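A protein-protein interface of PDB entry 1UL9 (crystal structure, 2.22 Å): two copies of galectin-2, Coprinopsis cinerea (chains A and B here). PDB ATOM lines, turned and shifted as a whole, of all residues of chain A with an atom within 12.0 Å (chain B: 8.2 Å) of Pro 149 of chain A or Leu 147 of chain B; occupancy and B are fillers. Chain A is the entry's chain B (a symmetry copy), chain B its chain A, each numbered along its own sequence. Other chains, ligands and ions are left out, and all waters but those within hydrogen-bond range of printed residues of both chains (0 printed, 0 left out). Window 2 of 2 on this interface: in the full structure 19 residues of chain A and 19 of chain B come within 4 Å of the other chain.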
ATOM      1  N   LEU A 144       0.807 -23.406 -13.709  1.00  0.00           N
ATOM      2  CA  LEU A 144       1.509 -23.031 -12.486  1.00  0.00           C
ATOM      3  C   LEU A 144       2.021 -21.598 -12.632  1.00  0.00           C
ATOM      4  O   LEU A 144       2.706 -21.277 -13.596  1.00  0.00           O
ATOM      5  CB  LEU A 144       2.696 -23.971 -12.253  1.00  0.00           C
ATOM      6  CG  LEU A 144       3.048 -24.393 -10.823  1.00  0.00           C
ATOM      7  CD1 LEU A 144       4.451 -24.985 -10.826  1.00  0.00           C
ATOM      8  CD2 LEU A 144       2.991 -23.216  -9.874  1.00  0.00           C
ATOM      9  N   PRO A 145       1.684 -20.715 -11.682  1.00  0.00           N
ATOM     10  CA  PRO A 145       2.151 -19.330 -11.775  1.00  0.00           C
ATOM     11  C   PRO A 145       3.578 -19.200 -11.245  1.00  0.00           C
ATOM     12  O   PRO A 145       4.105 -20.130 -10.628  1.00  0.00           O
ATOM     13  CB  PRO A 145       1.155 -18.581 -10.905  1.00  0.00           C
ATOM     14  CG  PRO A 145       0.917 -19.564  -9.790  1.00  0.00           C
ATOM     15  CD  PRO A 145       0.769 -20.885 -10.536  1.00  0.00           C
ATOM     16  N   PRO A 146       4.228 -18.051 -11.498  1.00  0.00           N
ATOM     17  CA  PRO A 146       5.595 -17.856 -11.012  1.00  0.00           C
ATOM     18  C   PRO A 146       5.615 -18.051  -9.504  1.00  0.00           C
ATOM     19  O   PRO A 146       4.675 -17.657  -8.816  1.00  0.00           O
ATOM     20  CB  PRO A 146       5.902 -16.425 -11.436  1.00  0.00           C
ATOM     21  CG  PRO A 146       5.176 -16.328 -12.746  1.00  0.00           C
ATOM     22  CD  PRO A 146       3.832 -16.950 -12.395  1.00  0.00           C
ATOM     23  N   LEU A 147       6.683 -18.654  -8.990  1.00  0.00           N
ATOM     24  CA  LEU A 147       6.772 -18.925  -7.561  1.00  0.00           C
ATOM     25  C   LEU A 147       7.605 -17.958  -6.729  1.00  0.00           C
ATOM     26  O   LEU A 147       8.685 -17.535  -7.135  1.00  0.00           O
ATOM     27  CB  LEU A 147       7.313 -20.339  -7.339  1.00  0.00           C
ATOM     28  CG  LEU A 147       6.606 -21.478  -8.075  1.00  0.00           C
ATOM     29  CD1 LEU A 147       7.331 -22.797  -7.780  1.00  0.00           C
ATOM     30  CD2 LEU A 147       5.147 -21.545  -7.641  1.00  0.00           C
ATOM     31  N   PRO A 148       7.104 -17.598  -5.541  1.00  0.00           N
ATOM     32  CA  PRO A 148       7.836 -16.686  -4.660  1.00  0.00           C
ATOM     33  C   PRO A 148       8.998 -17.476  -4.054  1.00  0.00           C
ATOM     34  O   PRO A 148       8.945 -18.703  -3.986  1.00  0.00           O
ATOM     35  CB  PRO A 148       6.788 -16.304  -3.623  1.00  0.00           C
ATOM     36  CG  PRO A 148       5.977 -17.561  -3.503  1.00  0.00           C
ATOM     37  CD  PRO A 148       5.799 -17.959  -4.958  1.00  0.00           C
ATOM     38  N   PRO A 149      10.063 -16.785  -3.612  1.00  0.00           N
ATOM     39  CA  PRO A 149      11.229 -17.448  -3.017  1.00  0.00           C
ATOM     40  C   PRO A 149      10.865 -18.352  -1.846  1.00  0.00           C
ATOM     41  O   PRO A 149      11.646 -19.213  -1.451  1.00  0.00           O
ATOM     42  CB  PRO A 149      12.105 -16.278  -2.575  1.00  0.00           C
ATOM     43  CG  PRO A 149      11.764 -15.204  -3.559  1.00  0.00           C
ATOM     44  CD  PRO A 149      10.258 -15.326  -3.656  1.00  0.00           C
ATOM     45  N   ALA A 150       9.676 -18.150  -1.291  1.00  0.00           N
ATOM     46  CA  ALA A 150       9.225 -18.941  -0.153  1.00  0.00           C
ATOM     47  C   ALA A 150       7.715 -18.797   0.050  1.00  0.00           C
ATOM     48  O   ALA A 150       7.120 -19.655   0.740  1.00  0.00           O
ATOM     49  CB  ALA A 150       9.976 -18.509   1.109  1.00  0.00           C
ATOM     50  OXT ALA A 150       7.145 -17.817  -0.479  1.00  0.00           O
ATOM     51  N   LEU B 144       5.103  -7.418   4.155  1.00  0.00           N
ATOM     52  CA  LEU B 144       5.195  -7.818   2.753  1.00  0.00           C
ATOM     53  C   LEU B 144       5.757  -9.229   2.644  1.00  0.00           C
ATOM     54  O   LEU B 144       6.846  -9.511   3.136  1.00  0.00           O
ATOM     55  CB  LEU B 144       6.110  -6.873   1.972  1.00  0.00           C
ATOM     56  CG  LEU B 144       5.564  -6.036   0.809  1.00  0.00           C
ATOM     57  CD1 LEU B 144       6.718  -5.791  -0.155  1.00  0.00           C
ATOM     58  CD2 LEU B 144       4.429  -6.733   0.085  1.00  0.00           C
ATOM     59  N   PRO B 145       5.020 -10.135   1.996  1.00  0.00           N
ATOM     60  CA  PRO B 145       5.500 -11.510   1.850  1.00  0.00           C
ATOM     61  C   PRO B 145       6.479 -11.583   0.683  1.00  0.00           C
ATOM     62  O   PRO B 145       6.580 -10.641  -0.110  1.00  0.00           O
ATOM     63  CB  PRO B 145       4.217 -12.286   1.576  1.00  0.00           C
ATOM     64  CG  PRO B 145       3.446 -11.315   0.730  1.00  0.00           C
ATOM     65  CD  PRO B 145       3.661  -9.988   1.448  1.00  0.00           C
ATOM     66  N   PRO B 146       7.223 -12.697   0.568  1.00  0.00           N
ATOM     67  CA  PRO B 146       8.181 -12.840  -0.531  1.00  0.00           C
ATOM     68  C   PRO B 146       7.461 -12.621  -1.853  1.00  0.00           C
ATOM     69  O   PRO B 146       6.269 -12.904  -1.970  1.00  0.00           O
ATOM     70  CB  PRO B 146       8.683 -14.267  -0.363  1.00  0.00           C
ATOM     71  CG  PRO B 146       8.638 -14.451   1.128  1.00  0.00           C
ATOM     72  CD  PRO B 146       7.293 -13.854   1.480  1.00  0.00           C
ATOM     73  N   LEU B 147       8.180 -12.120  -2.851  1.00  0.00           N
ATOM     74  CA  LEU B 147       7.564 -11.841  -4.137  1.00  0.00           C
ATOM     75  C   LEU B 147       7.978 -12.775  -5.268  1.00  0.00           C
ATOM     76  O   LEU B 147       9.157 -13.093  -5.435  1.00  0.00           O
ATOM     77  CB  LEU B 147       7.871 -10.397  -4.549  1.00  0.00           C
ATOM     78  CG  LEU B 147       7.561  -9.301  -3.527  1.00  0.00           C
ATOM     79  CD1 LEU B 147       8.003  -7.954  -4.097  1.00  0.00           C
ATOM     80  CD2 LEU B 147       6.065  -9.288  -3.196  1.00  0.00           C
ATOM     81  N   PRO B 148       7.002 -13.234  -6.061  1.00  0.00           N
ATOM     82  CA  PRO B 148       7.323 -14.124  -7.176  1.00  0.00           C
ATOM     83  C   PRO B 148       8.023 -13.276  -8.236  1.00  0.00           C
ATOM     84  O   PRO B 148       7.909 -12.053  -8.220  1.00  0.00           O
ATOM     85  CB  PRO B 148       5.951 -14.609  -7.628  1.00  0.00           C
ATOM     86  CG  PRO B 148       5.079 -13.424  -7.343  1.00  0.00           C
ATOM     87  CD  PRO B 148       5.551 -13.006  -5.969  1.00  0.00           C
ATOM     88  N   PRO B 149       8.761 -13.912  -9.159  1.00  0.00           N
ATOM     89  CA  PRO B 149       9.477 -13.200 -10.220  1.00  0.00           C
ATOM     90  C   PRO B 149       8.611 -12.204 -10.985  1.00  0.00           C
ATOM     91  O   PRO B 149       9.112 -11.215 -11.509  1.00  0.00           O
ATOM     92  CB  PRO B 149       9.968 -14.334 -11.114  1.00  0.00           C
ATOM     93  CG  PRO B 149      10.221 -15.420 -10.149  1.00  0.00           C
ATOM     94  CD  PRO B 149       9.006 -15.360  -9.255  1.00  0.00           C
ATOM     95  N   ALA B 150       7.311 -12.470 -11.047  1.00  0.00           N
ATOM     96  CA  ALA B 150       6.398 -11.590 -11.769  1.00  0.00           C
ATOM     97  C   ALA B 150       4.937 -11.837 -11.380  1.00  0.00           C
ATOM     98  O   ALA B 150       4.134 -10.881 -11.459  1.00  0.00           O
ATOM     99  CB  ALA B 150       6.584 -11.772 -13.277  1.00  0.00           C
ATOM    100  OXT ALA B 150       4.608 -12.988 -11.020  1.00  0.00           O
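Leu 144 of chain A touches none of the printed residues of chain B.
Printed residues of chain B within 4 Å of Pro 146 of chain A: Pro 148, Pro 149 and Ala 150.
Printed residues of chain B within 4 Å of Leu 147 of chain A: Pro 148 (3.7 Å) and Pro 149 (3.1 Å).
Printed residues of chain B within 4 Å of Pro 148 of chain A: Pro 146 (3.8 Å), Leu 147 (3.9 Å) and Pro 148 (3.6 Å).
Pro 149 of chain A touches two residues of chain B.
Of the printed residues of chain B, Ala 150 of chain A touches Pro 146.
No residue of chain A comes within 4 Å of Leu 144 of chain B.
No residue of chain A comes within 4 Å of Pro 145 of chain B.
Of the printed residues of chain A, Pro 146 of chain B touches Pro 148, Pro 149 and Ala 150.
Leu 147 of chain B touches two residues of chain A.
Pro 149 of chain B touches just these residues of chain A: Pro 146 and Leu 147.
Of the printed residues of chain A, Ala 150 of chain B touches Pro 146 (3.7 Å).
The nearest printed residue of chain B that does not touch Leu 147 of chain A is Leu 147 of chain B (4.8 Å).
Pro 146 of chain A touches Pro 148 of chain B.
Pro 149 of chain B touches Pro 146 of chain A (CD to CB, 3.9 Å).
CB of Pro 146 of chain A touches OXT of Ala 150 of chain B (3.7 Å).
CA of Pro 148 of chain B touches O of Leu 147 of chain A (3.7 Å).
CD of Pro 149 of chain B touches O of Leu 147 of chain A, at 3.1 Å.
O of Pro 146 of chain B touches CB of Pro 148 of chain A, at 3.8 Å.
Pro 148 of chain A touches Leu 147 of chain B (CA to O, 3.9 Å).
Pro 148 of chain B touches Pro 148 of chain A.
Pro 149 of chain A touches Pro 146 of chain B.
Pro 146 of chain B touches Ala 150 of chain A (CB to OXT, 3.9 Å).
Pro 146 of chain A touches Pro 148 of chain B, and with the chains exchanged Pro 148 of chain A touches Pro 146 of chain B.
Pro 146 of chain A touches Pro 149 of chain B, and with the chains exchanged Pro 149 of chain A touches Pro 146 of chain B.
Pro 146 of chain A touches Ala 150 of chain B, and with the chains exchanged Ala 150 of chain A touches Pro 146 of chain B.
Leu 147 of chain A touches Pro 148 of chain B, and with the chains exchanged Pro 148 of chain A touches Leu 147 of chain B.
Positions printed for both chains: 144, 145, 146, 147, 148, 149 and 150.
Hydrophobic or aromatic side chains of chain A within 4 Å of the printed part of chain B: Pro 146, Pro 148 and Pro 149.
Hydrophobic or aromatic side chains of chain B within 4 Å of the printed part of chain A: Pro 146, Pro 148 and Pro 149.
Among the printed residues, no Asp or Glu carboxylate lies within 4 Å of a Lys or Arg side-chain nitrogen of the other chain.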
